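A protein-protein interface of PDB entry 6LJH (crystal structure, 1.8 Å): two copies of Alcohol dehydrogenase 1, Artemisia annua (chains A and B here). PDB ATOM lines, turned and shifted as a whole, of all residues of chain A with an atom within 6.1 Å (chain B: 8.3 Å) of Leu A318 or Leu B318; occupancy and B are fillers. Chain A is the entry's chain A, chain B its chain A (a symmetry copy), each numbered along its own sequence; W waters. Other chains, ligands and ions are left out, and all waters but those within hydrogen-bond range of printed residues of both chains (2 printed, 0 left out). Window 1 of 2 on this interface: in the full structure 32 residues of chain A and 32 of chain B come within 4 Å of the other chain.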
ATOM      1  N   LEU A 280     -10.369   5.756  -8.958  1.00  0.00           N
ATOM      2  CA  LEU A 280      -9.371   4.704  -9.117  1.00  0.00           C
ATOM      3  C   LEU A 280      -8.069   5.105  -8.437  1.00  0.00           C
ATOM      4  O   LEU A 280      -7.467   4.320  -7.694  1.00  0.00           O
ATOM      5  CB  LEU A 280      -9.142   4.400 -10.600  1.00  0.00           C
ATOM      6  CG  LEU A 280      -7.960   3.456 -10.841  1.00  0.00           C
ATOM      7  CD1 LEU A 280      -8.264   2.121 -10.180  1.00  0.00           C
ATOM      8  CD2 LEU A 280      -7.703   3.270 -12.323  1.00  0.00           C
ATOM      9  N   LEU A 284      -6.247   3.324  -4.979  1.00  0.00           N
ATOM     10  CA  LEU A 284      -4.847   2.940  -4.865  1.00  0.00           C
ATOM     11  C   LEU A 284      -4.193   3.627  -3.670  1.00  0.00           C
ATOM     12  O   LEU A 284      -3.558   2.970  -2.834  1.00  0.00           O
ATOM     13  CB  LEU A 284      -4.123   3.258  -6.174  1.00  0.00           C
ATOM     14  CG  LEU A 284      -4.443   2.244  -7.286  1.00  0.00           C
ATOM     15  CD1 LEU A 284      -4.211   2.823  -8.690  1.00  0.00           C
ATOM     16  CD2 LEU A 284      -3.653   0.961  -7.077  1.00  0.00           C
ATOM     17  N   GLY A 292      -0.780  -3.735  -0.477  1.00  0.00           N
ATOM     18  CA  GLY A 292      -2.191  -3.493  -0.748  1.00  0.00           C
ATOM     19  C   GLY A 292      -2.601  -3.902  -2.155  1.00  0.00           C
ATOM     20  O   GLY A 292      -1.791  -3.928  -3.071  1.00  0.00           O
ATOM     21  N   THR A 293      -3.878  -4.263  -2.307  1.00  0.00           N
ATOM     22  CA  THR A 293      -4.439  -4.673  -3.595  1.00  0.00           C
ATOM     23  C   THR A 293      -5.671  -3.835  -3.882  1.00  0.00           C
ATOM     24  O   THR A 293      -6.460  -3.563  -2.975  1.00  0.00           O
ATOM     25  CB  THR A 293      -4.838  -6.170  -3.595  1.00  0.00           C
ATOM     26  OG1 THR A 293      -3.688  -6.977  -3.313  1.00  0.00           O
ATOM     27  CG2 THR A 293      -5.410  -6.593  -4.952  1.00  0.00           C
ATOM     28  N   VAL A 294      -5.841  -3.420  -5.140  1.00  0.00           N
ATOM     29  CA  VAL A 294      -7.049  -2.728  -5.573  1.00  0.00           C
ATOM     30  C   VAL A 294      -7.715  -3.555  -6.666  1.00  0.00           C
ATOM     31  O   VAL A 294      -7.040  -4.041  -7.579  1.00  0.00           O
ATOM     32  CB  VAL A 294      -6.741  -1.309  -6.089  1.00  0.00           C
ATOM     33  CG1 VAL A 294      -7.970  -0.711  -6.773  1.00  0.00           C
ATOM     34  CG2 VAL A 294      -6.279  -0.425  -4.953  1.00  0.00           C
ATOM     35  N   VAL A 295      -9.027  -3.718  -6.563  1.00  0.00           N
ATOM     36  CA  VAL A 295      -9.821  -4.347  -7.618  1.00  0.00           C
ATOM     37  C   VAL A 295     -10.795  -3.306  -8.147  1.00  0.00           C
ATOM     38  O   VAL A 295     -11.728  -2.918  -7.425  1.00  0.00           O
ATOM     39  CB  VAL A 295     -10.593  -5.574  -7.111  1.00  0.00           C
ATOM     40  CG1 VAL A 295     -11.407  -6.164  -8.261  1.00  0.00           C
ATOM     41  CG2 VAL A 295      -9.640  -6.602  -6.512  1.00  0.00           C
ATOM     42  N   PRO A 296     -10.627  -2.834  -9.382  1.00  0.00           N
ATOM     43  CA  PRO A 296     -11.538  -1.814  -9.912  1.00  0.00           C
ATOM     44  C   PRO A 296     -12.729  -2.449 -10.612  1.00  0.00           C
ATOM     45  O   PRO A 296     -12.639  -2.849 -11.774  1.00  0.00           O
ATOM     46  CB  PRO A 296     -10.652  -1.037 -10.895  1.00  0.00           C
ATOM     47  CG  PRO A 296      -9.679  -2.078 -11.403  1.00  0.00           C
ATOM     48  CD  PRO A 296      -9.475  -3.075 -10.280  1.00  0.00           C
ATOM     49  N   ILE A 307      -3.831   7.218 -13.958  1.00  0.00           N
ATOM     50  CA  ILE A 307      -3.255   6.828 -12.677  1.00  0.00           C
ATOM     51  C   ILE A 307      -2.077   7.749 -12.404  1.00  0.00           C
ATOM     52  O   ILE A 307      -1.223   7.925 -13.280  1.00  0.00           O
ATOM     53  CB  ILE A 307      -2.813   5.349 -12.705  1.00  0.00           C
ATOM     54  CG1 ILE A 307      -4.045   4.442 -12.767  1.00  0.00           C
ATOM     55  CG2 ILE A 307      -1.944   4.980 -11.509  1.00  0.00           C
ATOM     56  CD1 ILE A 307      -3.724   3.005 -13.081  1.00  0.00           C
ATOM     57  N   ARG A 316       1.943  -1.709  -4.930  1.00  0.00           N
ATOM     58  CA  ARG A 316       0.567  -2.177  -4.855  1.00  0.00           C
ATOM     59  C   ARG A 316       0.223  -3.075  -6.038  1.00  0.00           C
ATOM     60  O   ARG A 316       0.874  -3.055  -7.077  1.00  0.00           O
ATOM     61  CB  ARG A 316      -0.387  -0.978  -4.809  1.00  0.00           C
ATOM     62  CG  ARG A 316      -0.202  -0.132  -3.553  1.00  0.00           C
ATOM     63  CD  ARG A 316      -0.962   1.154  -3.669  1.00  0.00           C
ATOM     64  NE  ARG A 316      -0.979   1.920  -2.418  1.00  0.00           N
ATOM     65  CZ  ARG A 316      -0.461   3.137  -2.299  1.00  0.00           C
ATOM     66  NH1 ARG A 316       0.144   3.698  -3.337  1.00  0.00           N
ATOM     67  NH2 ARG A 316      -0.555   3.792  -1.153  1.00  0.00           N
ATOM     68  N   THR A 317      -0.821  -3.881  -5.865  1.00  0.00           N
ATOM     69  CA  THR A 317      -1.286  -4.782  -6.907  1.00  0.00           C
ATOM     70  C   THR A 317      -2.625  -4.273  -7.408  1.00  0.00           C
ATOM     71  O   THR A 317      -3.533  -4.031  -6.607  1.00  0.00           O
ATOM     72  CB  THR A 317      -1.427  -6.210  -6.377  1.00  0.00           C
ATOM     73  OG1 THR A 317      -0.139  -6.698  -5.982  1.00  0.00           O
ATOM     74  CG2 THR A 317      -2.026  -7.134  -7.444  1.00  0.00           C
ATOM     75  N   LEU A 318      -2.734  -4.088  -8.718  1.00  0.00           N
ATOM     76  CA  LEU A 318      -3.982  -3.671  -9.355  1.00  0.00           C
ATOM     77  C   LEU A 318      -4.489  -4.847 -10.187  1.00  0.00           C
ATOM     78  O   LEU A 318      -3.855  -5.231 -11.183  1.00  0.00           O
ATOM     79  CB  LEU A 318      -3.760  -2.426 -10.217  1.00  0.00           C
ATOM     80  CG  LEU A 318      -4.992  -1.802 -10.880  1.00  0.00           C
ATOM     81  CD1 LEU A 318      -6.070  -1.412  -9.849  1.00  0.00           C
ATOM     82  CD2 LEU A 318      -4.515  -0.563 -11.653  1.00  0.00           C
ATOM     83  N   LYS A 319      -5.610  -5.435  -9.765  1.00  0.00           N
ATOM     84  CA  LYS A 319      -6.126  -6.672 -10.354  1.00  0.00           C
ATOM     85  C   LYS A 319      -7.352  -6.357 -11.205  1.00  0.00           C
ATOM     86  O   LYS A 319      -8.423  -6.057 -10.672  1.00  0.00           O
ATOM     87  CB  LYS A 319      -6.458  -7.686  -9.258  1.00  0.00           C
ATOM     88  CG  LYS A 319      -6.971  -9.016  -9.774  1.00  0.00           C
ATOM     89  CD  LYS A 319      -5.925  -9.658 -10.678  1.00  0.00           C
ATOM     90  CE  LYS A 319      -6.331 -11.091 -11.053  1.00  0.00           C
ATOM     91  NZ  LYS A 319      -7.481 -11.087 -12.019  1.00  0.00           N
ATOM     92  N   PHE A 320      -7.199  -6.441 -12.526  1.00  0.00           N
ATOM     93  CA  PHE A 320      -8.332  -6.244 -13.421  1.00  0.00           C
ATOM     94  C   PHE A 320      -9.214  -7.491 -13.435  1.00  0.00           C
ATOM     95  O   PHE A 320      -8.809  -8.567 -12.991  1.00  0.00           O
ATOM     96  CB  PHE A 320      -7.832  -5.875 -14.814  1.00  0.00           C
ATOM     97  CG  PHE A 320      -6.937  -4.656 -14.815  1.00  0.00           C
ATOM     98  CD1 PHE A 320      -7.318  -3.499 -14.134  1.00  0.00           C
ATOM     99  CD2 PHE A 320      -5.713  -4.669 -15.472  1.00  0.00           C
ATOM    100  CE1 PHE A 320      -6.494  -2.363 -14.129  1.00  0.00           C
ATOM    101  CE2 PHE A 320      -4.866  -3.546 -15.457  1.00  0.00           C
ATOM    102  CZ  PHE A 320      -5.263  -2.390 -14.794  1.00  0.00           C
ATOM    103  N   GLU B 189       8.546  -9.566  -8.080  1.00  0.00           N
ATOM    104  CA  GLU B 189       7.292  -8.900  -8.436  1.00  0.00           C
ATOM    105  C   GLU B 189       6.313  -9.805  -9.163  1.00  0.00           C
ATOM    106  O   GLU B 189       5.102  -9.724  -8.933  1.00  0.00           O
ATOM    107  CB  GLU B 189       7.562  -7.658  -9.293  1.00  0.00           C
ATOM    108  CG  GLU B 189       8.463  -6.619  -8.601  1.00  0.00           C
ATOM    109  CD  GLU B 189       7.794  -5.929  -7.403  1.00  0.00           C
ATOM    110  OE1 GLU B 189       6.758  -6.418  -6.895  1.00  0.00           O
ATOM    111  OE2 GLU B 189       8.318  -4.880  -6.970  1.00  0.00           O
ATOM    112  N   CYS B 270       4.859  -9.624 -18.837  1.00  0.00           N
ATOM    113  CA  CYS B 270       5.411  -8.541 -19.635  1.00  0.00           C
ATOM    114  C   CYS B 270       6.044  -7.515 -18.700  1.00  0.00           C
ATOM    115  O   CYS B 270       5.478  -7.154 -17.661  1.00  0.00           O
ATOM    116  CB  CYS B 270       4.327  -7.914 -20.543  1.00  0.00           C
ATOM    117  SG  CYS B 270       4.947  -6.732 -21.777  1.00  0.00           S
ATOM    118  N   GLU B 272       7.737  -3.723 -18.608  1.00  0.00           N
ATOM    119  CA  GLU B 272       7.817  -2.468 -19.344  1.00  0.00           C
ATOM    120  C   GLU B 272       9.073  -1.748 -18.875  1.00  0.00           C
ATOM    121  O   GLU B 272       9.120  -1.245 -17.747  1.00  0.00           O
ATOM    122  CB  GLU B 272       6.560  -1.629 -19.116  1.00  0.00           C
ATOM    123  CG  GLU B 272       6.246  -0.661 -20.270  1.00  0.00           C
ATOM    124  CD  GLU B 272       7.429   0.222 -20.601  1.00  0.00           C
ATOM    125  OE1 GLU B 272       7.770   1.107 -19.769  1.00  0.00           O
ATOM    126  OE2 GLU B 272       8.034   0.009 -21.678  1.00  0.00           O
ATOM    127  N   LEU B 280       2.837   1.396 -21.721  1.00  0.00           N
ATOM    128  CA  LEU B 280       2.162   0.701 -20.629  1.00  0.00           C
ATOM    129  C   LEU B 280       0.919  -0.006 -21.146  1.00  0.00           C
ATOM    130  O   LEU B 280       0.679  -1.183 -20.844  1.00  0.00           O
ATOM    131  CB  LEU B 280       1.809   1.678 -19.507  1.00  0.00           C
ATOM    132  CG  LEU B 280       0.918   1.054 -18.429  1.00  0.00           C
ATOM    133  CD1 LEU B 280       1.679  -0.086 -17.770  1.00  0.00           C
ATOM    134  CD2 LEU B 280       0.504   2.084 -17.398  1.00  0.00           C
ATOM    135  N   ASN B 281       0.118   0.701 -21.946  1.00  0.00           N
ATOM    136  CA  ASN B 281      -1.054   0.090 -22.554  1.00  0.00           C
ATOM    137  C   ASN B 281      -0.668  -1.076 -23.448  1.00  0.00           C
ATOM    138  O   ASN B 281      -1.327  -2.120 -23.437  1.00  0.00           O
ATOM    139  CB  ASN B 281      -1.812   1.138 -23.362  1.00  0.00           C
ATOM    140  CG  ASN B 281      -3.286   0.874 -23.398  1.00  0.00           C
ATOM    141  OD1 ASN B 281      -3.978   1.020 -22.387  1.00  0.00           O
ATOM    142  ND2 ASN B 281      -3.786   0.476 -24.564  1.00  0.00           N
ATOM    143  N   ALA B 283       1.983  -2.994 -23.182  1.00  0.00           N
ATOM    144  CA  ALA B 283       2.436  -4.117 -22.357  1.00  0.00           C
ATOM    145  C   ALA B 283       1.255  -4.925 -21.843  1.00  0.00           C
ATOM    146  O   ALA B 283       1.286  -6.166 -21.830  1.00  0.00           O
ATOM    147  CB  ALA B 283       3.282  -3.608 -21.184  1.00  0.00           C
ATOM    148  N   LEU B 284       0.207  -4.235 -21.401  1.00  0.00           N
ATOM    149  CA  LEU B 284      -0.995  -4.919 -20.947  1.00  0.00           C
ATOM    150  C   LEU B 284      -1.630  -5.713 -22.084  1.00  0.00           C
ATOM    151  O   LEU B 284      -1.922  -6.907 -21.934  1.00  0.00           O
ATOM    152  CB  LEU B 284      -1.966  -3.899 -20.350  1.00  0.00           C
ATOM    153  CG  LEU B 284      -1.545  -3.434 -18.946  1.00  0.00           C
ATOM    154  CD1 LEU B 284      -2.137  -2.064 -18.581  1.00  0.00           C
ATOM    155  CD2 LEU B 284      -1.903  -4.489 -17.909  1.00  0.00           C
ATOM    156  N   SER B 287       0.114  -8.962 -22.833  1.00  0.00           N
ATOM    157  CA  SER B 287       0.060 -10.067 -21.888  1.00  0.00           C
ATOM    158  C   SER B 287      -1.274 -10.805 -22.026  1.00  0.00           C
ATOM    159  O   SER B 287      -2.256 -10.271 -22.541  1.00  0.00           O
ATOM    160  CB  SER B 287       0.248  -9.558 -20.449  1.00  0.00           C
ATOM    161  OG  SER B 287      -0.859  -8.758 -20.070  1.00  0.00           O
ATOM    162  N   GLY B 292      -2.322 -13.060 -17.439  1.00  0.00           N
ATOM    163  CA  GLY B 292      -1.093 -12.320 -17.691  1.00  0.00           C
ATOM    164  C   GLY B 292      -0.800 -11.279 -16.620  1.00  0.00           C
ATOM    165  O   GLY B 292      -1.697 -10.778 -15.957  1.00  0.00           O
ATOM    166  N   THR B 293       0.490 -10.984 -16.432  1.00  0.00           N
ATOM    167  CA  THR B 293       0.945  -9.998 -15.453  1.00  0.00           C
ATOM    168  C   THR B 293       1.835  -8.986 -16.151  1.00  0.00           C
ATOM    169  O   THR B 293       2.641  -9.357 -17.004  1.00  0.00           O
ATOM    170  CB  THR B 293       1.741 -10.659 -14.301  1.00  0.00           C
ATOM    171  OG1 THR B 293       0.921 -11.627 -13.638  1.00  0.00           O
ATOM    172  CG2 THR B 293       2.200  -9.621 -13.273  1.00  0.00           C
ATOM    173  N   VAL B 294       1.691  -7.707 -15.797  1.00  0.00           N
ATOM    174  CA  VAL B 294       2.578  -6.659 -16.290  1.00  0.00           C
ATOM    175  C   VAL B 294       3.277  -6.017 -15.099  1.00  0.00           C
ATOM    176  O   VAL B 294       2.636  -5.719 -14.085  1.00  0.00           O
ATOM    177  CB  VAL B 294       1.809  -5.594 -17.097  1.00  0.00           C
ATOM    178  CG1 VAL B 294       2.705  -4.388 -17.376  1.00  0.00           C
ATOM    179  CG2 VAL B 294       1.294  -6.186 -18.389  1.00  0.00           C
ATOM    180  N   VAL B 295       4.582  -5.815 -15.221  1.00  0.00           N
ATOM    181  CA  VAL B 295       5.353  -5.065 -14.232  1.00  0.00           C
ATOM    182  C   VAL B 295       5.906  -3.826 -14.919  1.00  0.00           C
ATOM    183  O   VAL B 295       6.789  -3.947 -15.782  1.00  0.00           O
ATOM    184  CB  VAL B 295       6.505  -5.893 -13.643  1.00  0.00           C
ATOM    185  CG1 VAL B 295       7.271  -5.040 -12.634  1.00  0.00           C
ATOM    186  CG2 VAL B 295       5.981  -7.177 -13.011  1.00  0.00           C
ATOM    187  N   PRO B 296       5.430  -2.630 -14.572  1.00  0.00           N
ATOM    188  CA  PRO B 296       5.928  -1.418 -15.232  1.00  0.00           C
ATOM    189  C   PRO B 296       7.130  -0.846 -14.497  1.00  0.00           C
ATOM    190  O   PRO B 296       6.983  -0.139 -13.500  1.00  0.00           O
ATOM    191  CB  PRO B 296       4.723  -0.470 -15.167  1.00  0.00           C
ATOM    192  CG  PRO B 296       4.017  -0.871 -13.892  1.00  0.00           C
ATOM    193  CD  PRO B 296       4.270  -2.352 -13.694  1.00  0.00           C
ATOM    194  N   ILE B 297       8.326  -1.162 -14.965  1.00  0.00           N
ATOM    195  CA  ILE B 297       9.539  -0.728 -14.283  1.00  0.00           C
ATOM    196  C   ILE B 297       9.956   0.672 -14.727  1.00  0.00           C
ATOM    197  O   ILE B 297      10.300   1.522 -13.903  1.00  0.00           O
ATOM    198  CB  ILE B 297      10.664  -1.754 -14.529  1.00  0.00           C
ATOM    199  CG1 ILE B 297      10.283  -3.134 -13.976  1.00  0.00           C
ATOM    200  CG2 ILE B 297      11.960  -1.252 -13.934  1.00  0.00           C
ATOM    201  CD1 ILE B 297      11.280  -4.251 -14.380  1.00  0.00           C
ATOM    202  N   VAL B 305      -0.521   8.507 -15.970  1.00  0.00           N
ATOM    203  CA  VAL B 305      -0.412   7.634 -17.132  1.00  0.00           C
ATOM    204  C   VAL B 305      -1.788   7.047 -17.417  1.00  0.00           C
ATOM    205  O   VAL B 305      -2.549   6.745 -16.492  1.00  0.00           O
ATOM    206  CB  VAL B 305       0.649   6.530 -16.920  1.00  0.00           C
ATOM    207  CG1 VAL B 305       0.317   5.698 -15.701  1.00  0.00           C
ATOM    208  CG2 VAL B 305       0.784   5.662 -18.176  1.00  0.00           C
ATOM    209  N   ILE B 307      -4.520   4.361 -19.080  1.00  0.00           N
ATOM    210  CA  ILE B 307      -4.763   2.962 -19.407  1.00  0.00           C
ATOM    211  C   ILE B 307      -6.098   2.887 -20.130  1.00  0.00           C
ATOM    212  O   ILE B 307      -7.089   3.447 -19.647  1.00  0.00           O
ATOM    213  CB  ILE B 307      -4.772   2.096 -18.129  1.00  0.00           C
ATOM    214  CG1 ILE B 307      -3.359   2.023 -17.545  1.00  0.00           C
ATOM    215  CG2 ILE B 307      -5.313   0.693 -18.382  1.00  0.00           C
ATOM    216  CD1 ILE B 307      -3.307   1.443 -16.156  1.00  0.00           C
ATOM    217  N   ILE B 311      -9.171  -2.425 -20.655  1.00  0.00           N
ATOM    218  CA  ILE B 311      -8.216  -3.348 -20.036  1.00  0.00           C
ATOM    219  C   ILE B 311      -8.641  -3.695 -18.616  1.00  0.00           C
ATOM    220  O   ILE B 311      -8.290  -4.776 -18.095  1.00  0.00           O
ATOM    221  CB  ILE B 311      -6.799  -2.737 -20.088  1.00  0.00           C
ATOM    222  CG1 ILE B 311      -6.323  -2.657 -21.543  1.00  0.00           C
ATOM    223  CG2 ILE B 311      -5.799  -3.568 -19.300  1.00  0.00           C
ATOM    224  CD1 ILE B 311      -5.038  -1.871 -21.716  1.00  0.00           C
ATOM    225  N   LEU B 312      -9.450  -2.831 -17.998  1.00  0.00           N
ATOM    226  CA  LEU B 312      -9.886  -3.082 -16.628  1.00  0.00           C
ATOM    227  C   LEU B 312     -10.786  -4.307 -16.525  1.00  0.00           C
ATOM    228  O   LEU B 312     -10.948  -4.838 -15.423  1.00  0.00           O
ATOM    229  CB  LEU B 312     -10.596  -1.842 -16.064  1.00  0.00           C
ATOM    230  CG  LEU B 312      -9.671  -0.854 -15.340  1.00  0.00           C
ATOM    231  CD1 LEU B 312      -8.570  -0.325 -16.264  1.00  0.00           C
ATOM    232  CD2 LEU B 312     -10.468   0.294 -14.759  1.00  0.00           C
ATOM    233  N   GLY B 315      -8.858  -9.105 -16.634  1.00  0.00           N
ATOM    234  CA  GLY B 315      -8.348 -10.120 -15.719  1.00  0.00           C
ATOM    235  C   GLY B 315      -6.852 -10.093 -15.491  1.00  0.00           C
ATOM    236  O   GLY B 315      -6.344 -10.899 -14.696  1.00  0.00           O
ATOM    237  N   ARG B 316      -6.138  -9.176 -16.135  1.00  0.00           N
ATOM    238  CA  ARG B 316      -4.691  -9.093 -16.006  1.00  0.00           C
ATOM    239  C   ARG B 316      -4.289  -8.503 -14.657  1.00  0.00           C
ATOM    240  O   ARG B 316      -5.067  -7.836 -13.985  1.00  0.00           O
ATOM    241  CB  ARG B 316      -4.116  -8.242 -17.143  1.00  0.00           C
ATOM    242  CG  ARG B 316      -4.340  -8.872 -18.515  1.00  0.00           C
ATOM    243  CD  ARG B 316      -3.999  -7.899 -19.602  1.00  0.00           C
ATOM    244  NE  ARG B 316      -4.011  -8.510 -20.936  1.00  0.00           N
ATOM    245  CZ  ARG B 316      -4.825  -8.122 -21.909  1.00  0.00           C
ATOM    246  NH1 ARG B 316      -5.711  -7.163 -21.682  1.00  0.00           N
ATOM    247  NH2 ARG B 316      -4.749  -8.684 -23.106  1.00  0.00           N
ATOM    248  N   THR B 317      -3.048  -8.768 -14.261  1.00  0.00           N
ATOM    249  CA  THR B 317      -2.510  -8.260 -13.008  1.00  0.00           C
ATOM    250  C   THR B 317      -1.459  -7.216 -13.334  1.00  0.00           C
ATOM    251  O   THR B 317      -0.546  -7.484 -14.122  1.00  0.00           O
ATOM    252  CB  THR B 317      -1.896  -9.388 -12.176  1.00  0.00           C
ATOM    253  OG1 THR B 317      -2.922 -10.321 -11.814  1.00  0.00           O
ATOM    254  CG2 THR B 317      -1.228  -8.834 -10.911  1.00  0.00           C
ATOM    255  N   LEU B 318      -1.602  -6.030 -12.755  1.00  0.00           N
ATOM    256  CA  LEU B 318      -0.631  -4.950 -12.917  1.00  0.00           C
ATOM    257  C   LEU B 318       0.054  -4.743 -11.568  1.00  0.00           C
ATOM    258  O   LEU B 318      -0.588  -4.314 -10.597  1.00  0.00           O
ATOM    259  CB  LEU B 318      -1.321  -3.671 -13.399  1.00  0.00           C
ATOM    260  CG  LEU B 318      -0.426  -2.466 -13.712  1.00  0.00           C
ATOM    261  CD1 LEU B 318       0.640  -2.797 -14.775  1.00  0.00           C
ATOM    262  CD2 LEU B 318      -1.342  -1.335 -14.202  1.00  0.00           C
ATOM    263  N   LYS B 319       1.346  -5.073 -11.499  1.00  0.00           N
ATOM    264  CA  LYS B 319       2.093  -5.092 -10.242  1.00  0.00           C
ATOM    265  C   LYS B 319       3.039  -3.897 -10.196  1.00  0.00           C
ATOM    266  O   LYS B 319       4.052  -3.872 -10.901  1.00  0.00           O
ATOM    267  CB  LYS B 319       2.856  -6.410 -10.096  1.00  0.00           C
ATOM    268  CG  LYS B 319       3.639  -6.537  -8.804  1.00  0.00           C
ATOM    269  CD  LYS B 319       2.692  -6.430  -7.613  1.00  0.00           C
ATOM    270  CE  LYS B 319       3.425  -6.754  -6.302  1.00  0.00           C
ATOM    271  NZ  LYS B 319       4.368  -5.649  -5.927  1.00  0.00           N
ATOM    272  N   PHE B 320       2.721  -2.915  -9.354  1.00  0.00           N
ATOM    273  CA  PHE B 320       3.606  -1.771  -9.173  1.00  0.00           C
ATOM    274  C   PHE B 320       4.790  -2.158  -8.289  1.00  0.00           C
ATOM    275  O   PHE B 320       4.775  -3.186  -7.610  1.00  0.00           O
ATOM    276  CB  PHE B 320       2.820  -0.595  -8.605  1.00  0.00           C
ATOM    277  CG  PHE B 320       1.629  -0.215  -9.456  1.00  0.00           C
ATOM    278  CD1 PHE B 320       1.768  -0.061 -10.836  1.00  0.00           C
ATOM    279  CD2 PHE B 320       0.375  -0.033  -8.888  1.00  0.00           C
ATOM    280  CE1 PHE B 320       0.668   0.292 -11.633  1.00  0.00           C
ATOM    281  CE2 PHE B 320      -0.742   0.297  -9.678  1.00  0.00           C
ATOM    282  CZ  PHE B 320      -0.589   0.470 -11.049  1.00  0.00           C
ATOM    283  N   THR B 321       5.837  -1.333  -8.321  1.00  0.00           N
ATOM    284  CA  THR B 321       7.156  -1.885  -8.038  1.00  0.00           C
ATOM    285  C   THR B 321       8.180  -0.765  -7.877  1.00  0.00           C
ATOM    286  O   THR B 321       8.175   0.201  -8.639  1.00  0.00           O
ATOM    287  CB  THR B 321       7.584  -2.823  -9.188  1.00  0.00           C
ATOM    288  OG1 THR B 321       8.950  -3.220  -9.003  1.00  0.00           O
ATOM    289  CG2 THR B 321       7.441  -2.121 -10.546  1.00  0.00           C
HETATM  290  O   HOH W   1      -7.491 -13.690 -13.262  1.00  0.00           O
HETATM  291  O   HOH W   2     -13.436  -3.845 -14.179  1.00  0.00           O
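N of Val A294 lies within hydrogen-bond range of O of Thr A317 (2.8 Å). The backbone carbonyl oxygen of Val A294 is in hydrogen-bond range of the backbone NH of Lys A319, at 3.0 Å. OE1 of Glu B189 is in salt-bridge range of NZ of Lys B319 (2.7 Å). The side-chain hydroxyl (OG) of Ser B287 is in hydrogen-bond range of the backbone carbonyl oxygen (O) of Leu B284. The backbone NH (N) of Val B294 lies within hydrogen-bond range of the backbone carbonyl oxygen (O) of Thr B317, at 2.8 Å. N of Lys B319 is in hydrogen-bond range of O of Val B294.
CD2 of Leu A284 touches CE2 of Phe B320 (3.96 Å). Ile B307 touches Ile A307. Lys B319 touches Arg A316 (CD to O, 3.9 Å). Thr A317 touches Thr B317. Leu B318 touches Thr A317 (O to C, 3.8 Å). CD of Lys B319 touches OG1 of Thr A317, 3.3 Å away. C of Thr B317 touches O of Leu A318, at 3.8 Å. Lys A319 touches Thr B317 (CD to OG1, 3.3 Å). Phe A320 touches Ile B311. Phe A320 touches Gly B315.
Printed residues of chain B within 4 Å of Thr A317: Thr B317 (3.9 Å), Leu B318 (3.8 Å) and Lys B319 (3.3 Å). Printed residues of chain B within 4 Å of Leu A318: Thr B317 and Leu B318. Gly B292 touches none of the printed residues of chain A. Printed residues of chain A within 4 Å of Ile B307: Ile A307. Printed residues of chain A within 4 Å of Thr B317: Thr A317, Leu A318 and Lys A319. Of the printed residues of chain A, Leu B318 touches Thr A317 and Leu A318. Printed residues of chain A within 4 Å of Lys B319: Arg A316 and Thr A317. The nearest printed residue of chain A that does not touch Leu B318 is Arg A316 (4.01 Å). The nearest printed residue of chain B that does not touch Thr A317 is Phe B320 (5.0 Å).
The backbone carbonyl oxygen (O) of Ile A307 sits at hydrogen-bond distance from the backbone NH (N) of Val B305, at 2.8 Å. The backbone carbonyl oxygen of Arg A316 lies within hydrogen-bond range of the backbone NH of Phe B320, 2.9 Å away. The backbone NH (N) of Leu B318 is in hydrogen-bond range of the backbone carbonyl oxygen (O) of Leu A318. O of Gly B315 is in hydrogen-bond range of NZ of Lys A319 (2.9 Å). N of Phe A320 lies within hydrogen-bond range of O of Arg B316 (2.9 Å).
Thr A317 touches its own counterpart, Thr B317. Thr A317 touches Leu B318, and with the chains exchanged Leu A318 touches Thr B317. Thr A317 touches Lys B319, and with the chains exchanged Lys A319 touches Thr B317. Leu B318 touches its own counterpart, Leu A318. Positions printed for both chains: 280, 284, 292, 293, 294, 295, 296, 307, 316, 317, 318, 319 and 320.
Water W2 lies within hydrogen-bond range of O of Pro A296 (2.7 Å) and O of Leu B312 (3.0 Å). Water W1 lies within hydrogen-bond range of NZ of Lys A319 (2.9 Å) and O of Gly B315 (3.3 Å).
Printed residues of chain B that touch a printed residue of chain A: Leu B284, Val B305, Ile B307, Ile B311, Leu B312, Gly B315, Arg B316, Thr B317, Leu B318, Lys B319 and Phe B320. Hydrophobic or aromatic side chains of chain A that line the printed part of chain B: Leu A284, Ile A307, Leu A318 and Phe A320. Among the printed residues, 18 pairs touch across the chains.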
